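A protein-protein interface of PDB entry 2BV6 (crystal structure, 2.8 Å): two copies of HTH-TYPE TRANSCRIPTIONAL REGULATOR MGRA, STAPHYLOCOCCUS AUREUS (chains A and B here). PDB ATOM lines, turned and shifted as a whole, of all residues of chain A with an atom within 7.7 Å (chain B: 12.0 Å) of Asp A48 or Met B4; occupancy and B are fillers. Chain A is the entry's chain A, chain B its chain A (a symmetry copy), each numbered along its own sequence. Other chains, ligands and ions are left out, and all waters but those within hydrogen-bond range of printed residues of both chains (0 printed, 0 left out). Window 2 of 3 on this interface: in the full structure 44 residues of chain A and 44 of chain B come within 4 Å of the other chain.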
ATOM      1  N   VAL A  42      -6.765  12.217 -24.413  1.00  0.00           N
ATOM      2  CA  VAL A  42      -6.193  13.469 -23.935  1.00  0.00           C
ATOM      3  C   VAL A  42      -7.020  14.637 -24.463  1.00  0.00           C
ATOM      4  O   VAL A  42      -7.436  15.508 -23.700  1.00  0.00           O
ATOM      5  CB  VAL A  42      -4.726  13.629 -24.401  1.00  0.00           C
ATOM      6  CG1 VAL A  42      -4.267  15.065 -24.219  1.00  0.00           C
ATOM      7  CG2 VAL A  42      -3.829  12.695 -23.611  1.00  0.00           C
ATOM      8  N   LEU A  43      -7.264  14.655 -25.767  1.00  0.00           N
ATOM      9  CA  LEU A  43      -8.046  15.735 -26.355  1.00  0.00           C
ATOM     10  C   LEU A  43      -9.412  15.781 -25.716  1.00  0.00           C
ATOM     11  O   LEU A  43      -9.976  16.847 -25.499  1.00  0.00           O
ATOM     12  CB  LEU A  43      -8.208  15.528 -27.856  1.00  0.00           C
ATOM     13  CG  LEU A  43      -6.916  15.525 -28.661  1.00  0.00           C
ATOM     14  CD1 LEU A  43      -7.283  15.450 -30.129  1.00  0.00           C
ATOM     15  CD2 LEU A  43      -6.100  16.786 -28.388  1.00  0.00           C
ATOM     16  N   THR A  44      -9.939  14.601 -25.424  1.00  0.00           N
ATOM     17  CA  THR A  44     -11.246  14.485 -24.817  1.00  0.00           C
ATOM     18  C   THR A  44     -11.217  15.281 -23.536  1.00  0.00           C
ATOM     19  O   THR A  44     -12.116  16.083 -23.271  1.00  0.00           O
ATOM     20  CB  THR A  44     -11.573  13.025 -24.505  1.00  0.00           C
ATOM     21  OG1 THR A  44     -11.485  12.249 -25.713  1.00  0.00           O
ATOM     22  CG2 THR A  44     -12.970  12.913 -23.914  1.00  0.00           C
ATOM     23  N   ILE A  45     -10.176  15.060 -22.738  1.00  0.00           N
ATOM     24  CA  ILE A  45     -10.028  15.795 -21.495  1.00  0.00           C
ATOM     25  C   ILE A  45      -9.903  17.293 -21.787  1.00  0.00           C
ATOM     26  O   ILE A  45     -10.548  18.110 -21.143  1.00  0.00           O
ATOM     27  CB  ILE A  45      -8.783  15.346 -20.732  1.00  0.00           C
ATOM     28  CG1 ILE A  45      -8.968  13.914 -20.253  1.00  0.00           C
ATOM     29  CG2 ILE A  45      -8.532  16.257 -19.539  1.00  0.00           C
ATOM     30  CD1 ILE A  45      -7.832  13.422 -19.384  1.00  0.00           C
ATOM     31  N   LEU A  46      -9.085  17.654 -22.764  1.00  0.00           N
ATOM     32  CA  LEU A  46      -8.913  19.058 -23.081  1.00  0.00           C
ATOM     33  C   LEU A  46     -10.137  19.725 -23.660  1.00  0.00           C
ATOM     34  O   LEU A  46     -10.304  20.941 -23.513  1.00  0.00           O
ATOM     35  CB  LEU A  46      -7.762  19.260 -24.056  1.00  0.00           C
ATOM     36  CG  LEU A  46      -6.361  19.208 -23.462  1.00  0.00           C
ATOM     37  CD1 LEU A  46      -5.349  19.399 -24.576  1.00  0.00           C
ATOM     38  CD2 LEU A  46      -6.216  20.285 -22.387  1.00  0.00           C
ATOM     39  N   TRP A  47     -10.988  18.956 -24.336  1.00  0.00           N
ATOM     40  CA  TRP A  47     -12.186  19.547 -24.930  1.00  0.00           C
ATOM     41  C   TRP A  47     -13.161  19.897 -23.844  1.00  0.00           C
ATOM     42  O   TRP A  47     -14.021  20.761 -24.015  1.00  0.00           O
ATOM     43  CB  TRP A  47     -12.837  18.601 -25.925  1.00  0.00           C
ATOM     44  CG  TRP A  47     -12.110  18.555 -27.207  1.00  0.00           C
ATOM     45  CD1 TRP A  47     -11.576  19.612 -27.879  1.00  0.00           C
ATOM     46  CD2 TRP A  47     -11.854  17.400 -28.002  1.00  0.00           C
ATOM     47  NE1 TRP A  47     -11.004  19.188 -29.047  1.00  0.00           N
ATOM     48  CE2 TRP A  47     -11.159  17.833 -29.150  1.00  0.00           C
ATOM     49  CE3 TRP A  47     -12.145  16.040 -27.858  1.00  0.00           C
ATOM     50  CZ2 TRP A  47     -10.746  16.954 -30.148  1.00  0.00           C
ATOM     51  CZ3 TRP A  47     -11.734  15.165 -28.850  1.00  0.00           C
ATOM     52  CH2 TRP A  47     -11.042  15.628 -29.983  1.00  0.00           C
ATOM     53  N   ASP A  48     -13.005  19.221 -22.715  1.00  0.00           N
ATOM     54  CA  ASP A  48     -13.852  19.458 -21.570  1.00  0.00           C
ATOM     55  C   ASP A  48     -13.248  20.569 -20.701  1.00  0.00           C
ATOM     56  O   ASP A  48     -13.983  21.312 -20.051  1.00  0.00           O
ATOM     57  CB  ASP A  48     -14.001  18.156 -20.773  1.00  0.00           C
ATOM     58  CG  ASP A  48     -14.832  18.332 -19.514  1.00  0.00           C
ATOM     59  OD1 ASP A  48     -14.317  18.870 -18.512  1.00  0.00           O
ATOM     60  OD2 ASP A  48     -16.014  17.936 -19.525  1.00  0.00           O
ATOM     61  N   GLU A  49     -11.919  20.697 -20.711  1.00  0.00           N
ATOM     62  CA  GLU A  49     -11.247  21.712 -19.898  1.00  0.00           C
ATOM     63  C   GLU A  49     -10.139  22.469 -20.625  1.00  0.00           C
ATOM     64  O   GLU A  49      -9.034  21.958 -20.768  1.00  0.00           O
ATOM     65  CB  GLU A  49     -10.675  21.065 -18.639  1.00  0.00           C
ATOM     66  CG  GLU A  49     -10.438  22.069 -17.550  1.00  0.00           C
ATOM     67  CD  GLU A  49     -11.603  23.034 -17.435  1.00  0.00           C
ATOM     68  OE1 GLU A  49     -12.674  22.620 -16.935  1.00  0.00           O
ATOM     69  OE2 GLU A  49     -11.449  24.200 -17.864  1.00  0.00           O
ATOM     70  N   SER A  50     -10.452  23.702 -21.041  1.00  0.00           N
ATOM     71  CA  SER A  50      -9.546  24.580 -21.800  1.00  0.00           C
ATOM     72  C   SER A  50      -8.085  24.241 -21.564  1.00  0.00           C
ATOM     73  O   SER A  50      -7.460  23.653 -22.466  1.00  0.00           O
ATOM     74  CB  SER A  50      -9.867  26.065 -21.519  1.00  0.00           C
ATOM     75  OG  SER A  50     -11.101  26.463 -22.124  1.00  0.00           O
ATOM     76  N   PRO A  51      -7.490  24.681 -20.422  1.00  0.00           N
ATOM     77  CA  PRO A  51      -6.085  24.335 -20.139  1.00  0.00           C
ATOM     78  C   PRO A  51      -6.160  23.430 -18.917  1.00  0.00           C
ATOM     79  O   PRO A  51      -6.972  23.649 -18.015  1.00  0.00           O
ATOM     80  CB  PRO A  51      -5.429  25.674 -19.823  1.00  0.00           C
ATOM     81  CG  PRO A  51      -6.468  26.368 -19.101  1.00  0.00           C
ATOM     82  CD  PRO A  51      -7.813  25.959 -19.762  1.00  0.00           C
ATOM     83  N   VAL A  52      -5.345  22.396 -18.877  1.00  0.00           N
ATOM     84  CA  VAL A  52      -5.420  21.511 -17.730  1.00  0.00           C
ATOM     85  C   VAL A  52      -4.030  21.103 -17.245  1.00  0.00           C
ATOM     86  O   VAL A  52      -3.066  21.101 -18.009  1.00  0.00           O
ATOM     87  CB  VAL A  52      -6.296  20.261 -18.084  1.00  0.00           C
ATOM     88  CG1 VAL A  52      -5.529  19.281 -18.985  1.00  0.00           C
ATOM     89  CG2 VAL A  52      -6.765  19.597 -16.822  1.00  0.00           C
ATOM     90  N   LYS A  56      -3.621  15.794 -14.327  1.00  0.00           N
ATOM     91  CA  LYS A  56      -4.943  15.248 -14.577  1.00  0.00           C
ATOM     92  C   LYS A  56      -4.890  14.185 -15.677  1.00  0.00           C
ATOM     93  O   LYS A  56      -5.608  13.183 -15.624  1.00  0.00           O
ATOM     94  CB  LYS A  56      -5.935  16.333 -14.974  1.00  0.00           C
ATOM     95  CG  LYS A  56      -7.289  15.739 -15.286  1.00  0.00           C
ATOM     96  CD  LYS A  56      -8.449  16.694 -15.032  1.00  0.00           C
ATOM     97  CE  LYS A  56      -9.793  15.958 -15.185  1.00  0.00           C
ATOM     98  NZ  LYS A  56     -10.993  16.838 -15.047  1.00  0.00           N
ATOM     99  N   GLU A  60      -6.380  10.450 -15.174  1.00  0.00           N
ATOM    100  CA  GLU A  60      -7.445   9.840 -15.957  1.00  0.00           C
ATOM    101  C   GLU A  60      -7.031   8.697 -16.869  1.00  0.00           C
ATOM    102  O   GLU A  60      -7.876   8.010 -17.441  1.00  0.00           O
ATOM    103  CB  GLU A  60      -8.143  10.914 -16.775  1.00  0.00           C
ATOM    104  CG  GLU A  60      -8.559  12.107 -15.944  1.00  0.00           C
ATOM    105  CD  GLU A  60      -9.458  11.732 -14.781  1.00  0.00           C
ATOM    106  OE1 GLU A  60     -10.634  11.390 -15.021  1.00  0.00           O
ATOM    107  OE2 GLU A  60      -8.987  11.775 -13.624  1.00  0.00           O
ATOM    108  N   LEU A  97      -5.258  23.418 -25.552  1.00  0.00           N
ATOM    109  CA  LEU A  97      -5.760  22.988 -26.854  1.00  0.00           C
ATOM    110  C   LEU A  97      -5.131  23.928 -27.870  1.00  0.00           C
ATOM    111  O   LEU A  97      -4.758  25.055 -27.536  1.00  0.00           O
ATOM    112  CB  LEU A  97      -7.277  23.140 -26.933  1.00  0.00           C
ATOM    113  CG  LEU A  97      -8.066  21.901 -26.542  1.00  0.00           C
ATOM    114  CD1 LEU A  97      -9.522  22.225 -26.324  1.00  0.00           C
ATOM    115  CD2 LEU A  97      -7.887  20.870 -27.641  1.00  0.00           C
ATOM    116  N   ARG A 105     -12.616  18.979 -32.459  1.00  0.00           N
ATOM    117  CA  ARG A 105     -13.661  18.899 -31.436  1.00  0.00           C
ATOM    118  C   ARG A 105     -14.999  18.269 -31.831  1.00  0.00           C
ATOM    119  O   ARG A 105     -15.421  17.286 -31.223  1.00  0.00           O
ATOM    120  CB  ARG A 105     -13.936  20.277 -30.820  1.00  0.00           C
ATOM    121  CG  ARG A 105     -14.907  20.212 -29.638  1.00  0.00           C
ATOM    122  CD  ARG A 105     -15.393  21.590 -29.219  1.00  0.00           C
ATOM    123  NE  ARG A 105     -14.326  22.418 -28.666  1.00  0.00           N
ATOM    124  CZ  ARG A 105     -13.848  22.307 -27.428  1.00  0.00           C
ATOM    125  NH1 ARG A 105     -14.344  21.403 -26.591  1.00  0.00           N
ATOM    126  NH2 ARG A 105     -12.856  23.091 -27.030  1.00  0.00           N
ATOM    127  N   SER A 109     -15.875  14.677 -29.920  1.00  0.00           N
ATOM    128  CA  SER A 109     -16.321  15.035 -28.579  1.00  0.00           C
ATOM    129  C   SER A 109     -17.486  14.187 -28.067  1.00  0.00           C
ATOM    130  O   SER A 109     -17.614  13.974 -26.859  1.00  0.00           O
ATOM    131  CB  SER A 109     -16.692  16.513 -28.533  1.00  0.00           C
ATOM    132  OG  SER A 109     -17.710  16.788 -29.467  1.00  0.00           O
ATOM    133  N   SER A 112     -17.915   8.814 -26.527  1.00  0.00           N
ATOM    134  CA  SER A 112     -18.418   7.843 -25.560  1.00  0.00           C
ATOM    135  C   SER A 112     -19.899   7.501 -25.728  1.00  0.00           C
ATOM    136  O   SER A 112     -20.423   6.619 -25.044  1.00  0.00           O
ATOM    137  CB  SER A 112     -18.135   8.301 -24.124  1.00  0.00           C
ATOM    138  OG  SER A 112     -16.898   7.772 -23.659  1.00  0.00           O
ATOM    139  N   ASP A 113     -20.574   8.187 -26.645  1.00  0.00           N
ATOM    140  CA  ASP A 113     -21.983   7.910 -26.890  1.00  0.00           C
ATOM    141  C   ASP A 113     -22.219   7.341 -28.276  1.00  0.00           C
ATOM    142  O   ASP A 113     -23.110   6.513 -28.458  1.00  0.00           O
ATOM    143  CB  ASP A 113     -22.816   9.163 -26.655  1.00  0.00           C
ATOM    144  CG  ASP A 113     -23.004   9.440 -25.185  1.00  0.00           C
ATOM    145  OD1 ASP A 113     -23.613   8.588 -24.500  1.00  0.00           O
ATOM    146  OD2 ASP A 113     -22.533  10.494 -24.710  1.00  0.00           O
ATOM    147  N   MET B   4     -16.843  17.226 -16.669  1.00  0.00           N
ATOM    148  CA  MET B   4     -17.739  16.049 -16.825  1.00  0.00           C
ATOM    149  C   MET B   4     -17.260  14.927 -15.913  1.00  0.00           C
ATOM    150  O   MET B   4     -16.244  15.053 -15.225  1.00  0.00           O
ATOM    151  CB  MET B   4     -17.725  15.560 -18.281  1.00  0.00           C
ATOM    152  CG  MET B   4     -16.497  14.711 -18.667  1.00  0.00           C
ATOM    153  SD  MET B   4     -16.291  14.393 -20.592  1.00  0.00           S
ATOM    154  CE  MET B   4     -18.159  14.145 -21.060  1.00  0.00           C
ATOM    155  N   ASN B   5     -18.002  13.829 -15.909  1.00  0.00           N
ATOM    156  CA  ASN B   5     -17.635  12.683 -15.099  1.00  0.00           C
ATOM    157  C   ASN B   5     -17.025  11.674 -16.055  1.00  0.00           C
ATOM    158  O   ASN B   5     -17.701  11.195 -16.967  1.00  0.00           O
ATOM    159  CB  ASN B   5     -18.874  12.086 -14.425  1.00  0.00           C
ATOM    160  CG  ASN B   5     -18.522  11.126 -13.301  1.00  0.00           C
ATOM    161  OD1 ASN B   5     -17.346  10.941 -12.974  1.00  0.00           O
ATOM    162  ND2 ASN B   5     -19.541  10.517 -12.697  1.00  0.00           N
ATOM    163  N   LEU B   6     -15.747  11.365 -15.860  1.00  0.00           N
ATOM    164  CA  LEU B   6     -15.071  10.409 -16.727  1.00  0.00           C
ATOM    165  C   LEU B   6     -15.376   8.975 -16.328  1.00  0.00           C
ATOM    166  O   LEU B   6     -15.135   8.046 -17.097  1.00  0.00           O
ATOM    167  CB  LEU B   6     -13.558  10.658 -16.730  1.00  0.00           C
ATOM    168  CG  LEU B   6     -13.166  11.988 -17.388  1.00  0.00           C
ATOM    169  CD1 LEU B   6     -11.659  12.097 -17.483  1.00  0.00           C
ATOM    170  CD2 LEU B   6     -13.787  12.084 -18.780  1.00  0.00           C
ATOM    171  N   LYS B   7     -15.897   8.791 -15.121  1.00  0.00           N
ATOM    172  CA  LYS B   7     -16.263   7.454 -14.682  1.00  0.00           C
ATOM    173  C   LYS B   7     -17.456   7.081 -15.555  1.00  0.00           C
ATOM    174  O   LYS B   7     -17.713   5.904 -15.813  1.00  0.00           O
ATOM    175  CB  LYS B   7     -16.660   7.458 -13.202  1.00  0.00           C
ATOM    176  CG  LYS B   7     -15.508   7.745 -12.254  1.00  0.00           C
ATOM    177  CD  LYS B   7     -15.950   7.677 -10.804  1.00  0.00           C
ATOM    178  CE  LYS B   7     -14.787   7.946  -9.855  1.00  0.00           C
ATOM    179  NZ  LYS B   7     -15.228   7.963  -8.427  1.00  0.00           N
ATOM    180  N   GLU B   8     -18.160   8.113 -16.022  1.00  0.00           N
ATOM    181  CA  GLU B   8     -19.329   7.955 -16.881  1.00  0.00           C
ATOM    182  C   GLU B   8     -18.930   7.798 -18.337  1.00  0.00           C
ATOM    183  O   GLU B   8     -19.773   7.528 -19.194  1.00  0.00           O
ATOM    184  CB  GLU B   8     -20.249   9.170 -16.775  1.00  0.00           C
ATOM    185  CG  GLU B   8     -20.802   9.436 -15.393  1.00  0.00           C
ATOM    186  CD  GLU B   8     -21.523   8.237 -14.804  1.00  0.00           C
ATOM    187  OE1 GLU B   8     -21.829   7.279 -15.557  1.00  0.00           O
ATOM    188  OE2 GLU B   8     -21.790   8.261 -13.581  1.00  0.00           O
ATOM    189  N   GLN B   9     -17.646   7.980 -18.618  1.00  0.00           N
ATOM    190  CA  GLN B   9     -17.161   7.865 -19.981  1.00  0.00           C
ATOM    191  C   GLN B   9     -16.694   6.461 -20.320  1.00  0.00           C
ATOM    192  O   GLN B   9     -15.615   6.033 -19.903  1.00  0.00           O
ATOM    193  CB  GLN B   9     -16.036   8.862 -20.215  1.00  0.00           C
ATOM    194  CG  GLN B   9     -16.464  10.279 -19.933  1.00  0.00           C
ATOM    195  CD  GLN B   9     -17.792  10.601 -20.582  1.00  0.00           C
ATOM    196  OE1 GLN B   9     -17.947  10.457 -21.795  1.00  0.00           O
ATOM    197  NE2 GLN B   9     -18.761  11.038 -19.778  1.00  0.00           N
ATOM    198  N   LEU B  10     -17.527   5.751 -21.075  1.00  0.00           N
ATOM    199  CA  LEU B  10     -17.225   4.391 -21.499  1.00  0.00           C
ATOM    200  C   LEU B  10     -15.859   4.330 -22.152  1.00  0.00           C
ATOM    201  O   LEU B  10     -15.064   3.423 -21.883  1.00  0.00           O
ATOM    202  CB  LEU B  10     -18.264   3.903 -22.505  1.00  0.00           C
ATOM    203  CG  LEU B  10     -19.444   3.094 -21.985  1.00  0.00           C
ATOM    204  CD1 LEU B  10     -20.267   2.651 -23.182  1.00  0.00           C
ATOM    205  CD2 LEU B  10     -18.957   1.884 -21.195  1.00  0.00           C
ATOM    206  N   CYS B  11     -15.598   5.292 -23.026  1.00  0.00           N
ATOM    207  CA  CYS B  11     -14.329   5.327 -23.701  1.00  0.00           C
ATOM    208  C   CYS B  11     -13.197   5.206 -22.702  1.00  0.00           C
ATOM    209  O   CYS B  11     -12.271   4.426 -22.913  1.00  0.00           O
ATOM    210  CB  CYS B  11     -14.204   6.603 -24.515  1.00  0.00           C
ATOM    211  SG  CYS B  11     -15.043   6.476 -26.114  1.00  0.00           S
ATOM    212  N   PHE B  12     -13.281   5.951 -21.604  1.00  0.00           N
ATOM    213  CA  PHE B  12     -12.245   5.902 -20.578  1.00  0.00           C
ATOM    214  C   PHE B  12     -12.335   4.620 -19.770  1.00  0.00           C
ATOM    215  O   PHE B  12     -11.316   4.029 -19.416  1.00  0.00           O
ATOM    216  CB  PHE B  12     -12.345   7.117 -19.646  1.00  0.00           C
ATOM    217  CG  PHE B  12     -11.924   8.414 -20.290  1.00  0.00           C
ATOM    218  CD1 PHE B  12     -12.831   9.180 -21.014  1.00  0.00           C
ATOM    219  CD2 PHE B  12     -10.605   8.853 -20.201  1.00  0.00           C
ATOM    220  CE1 PHE B  12     -12.431  10.365 -21.644  1.00  0.00           C
ATOM    221  CE2 PHE B  12     -10.194  10.036 -20.827  1.00  0.00           C
ATOM    222  CZ  PHE B  12     -11.109  10.792 -21.550  1.00  0.00           C
ATOM    223  N   SER B  13     -13.559   4.187 -19.492  1.00  0.00           N
ATOM    224  CA  SER B  13     -13.793   2.963 -18.721  1.00  0.00           C
ATOM    225  C   SER B  13     -13.181   1.726 -19.384  1.00  0.00           C
ATOM    226  O   SER B  13     -12.412   0.995 -18.750  1.00  0.00           O
ATOM    227  CB  SER B  13     -15.297   2.756 -18.505  1.00  0.00           C
ATOM    228  OG  SER B  13     -15.842   3.796 -17.701  1.00  0.00           O
ATOM    229  N   ASN B  16      -9.257   2.011 -19.770  1.00  0.00           N
ATOM    230  CA  ASN B  16      -8.621   1.792 -18.486  1.00  0.00           C
ATOM    231  C   ASN B  16      -8.767   0.405 -17.900  1.00  0.00           C
ATOM    232  O   ASN B  16      -7.807  -0.131 -17.336  1.00  0.00           O
ATOM    233  CB  ASN B  16      -9.105   2.832 -17.478  1.00  0.00           C
ATOM    234  CG  ASN B  16      -8.443   4.176 -17.686  1.00  0.00           C
ATOM    235  OD1 ASN B  16      -7.213   4.271 -17.732  1.00  0.00           O
ATOM    236  ND2 ASN B  16      -9.251   5.225 -17.811  1.00  0.00           N
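The side-chain carboxylate of Asp A48 lies within hydrogen-bond range of the backbone NH of Met B4 (3.1 Å). O of Glu A60 is in hydrogen-bond range of ND2 of Asn B16 (3.1 Å). OE1 of Gln B9 sits close to OG of Ser A112 (3.4 Å). The side-chain hydroxyl of Ser A112 is in hydrogen-bond range of the backbone NH of Leu B10 (3.3 Å). The backbone NH (N) of Cys B11 is in hydrogen-bond range of the side-chain hydroxyl (OG) of Ser A112, at 2.9 Å.
The side-chain amide nitrogen (NE2) of Gln B9 sits at hydrogen-bond distance from the backbone carbonyl oxygen (O) of Asn B5 (3.0 Å). The backbone carbonyl oxygen (O) of Gln B9 sits at hydrogen-bond distance from the side-chain hydroxyl (OG) of Ser B13. O of Phe B12 sits at hydrogen-bond distance from ND2 of Asn B16, at 2.9 Å.
Thr A44 touches Phe B12. Glu A60 touches Leu B6. Glu A60 touches Phe B12 (O to CD2, 3.97 Å).
Of chain B, only Met B4 comes within 4 Å of Asp A48. Met B4 touches just one residue of chain A: Asp A48 (3.1 Å). No residue of chain B comes within 4 Å of Leu A46. No residue of chain B comes within 4 Å of Glu A49. No residue of chain B comes within 4 Å of Ser A50. Of the printed residues of chain A, Asn B16 touches Glu A60 (3.1 Å). Of the printed residues of chain A, Leu B10 touches Ser A112 (3.3 Å). Pro A51 touches none of the printed residues of chain B. The nearest residue of chain B that does not touch Asp A48 is Asn B5 (5.8 Å). The nearest residue of chain A that does not touch Met B4 is Thr A44 (4.9 Å). The nearest printed residue of chain A that does not touch Phe B12 is Ile A45 (4.002 Å).
Hydrophobic or aromatic side chains of chain B that line the printed part of chain A: Met B4, Leu B6 and Phe B12. Among the printed residues, 8 pairs touch across the chains. Among the printed residues, no Asp or Glu carboxylate lies within 4 Å of a Lys or Arg side-chain nitrogen of the other chain.
No position is printed for both chains. Of the 8 pairs that touch across the chains among the printed residues, none has its exchanged pair printed and touching as well.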
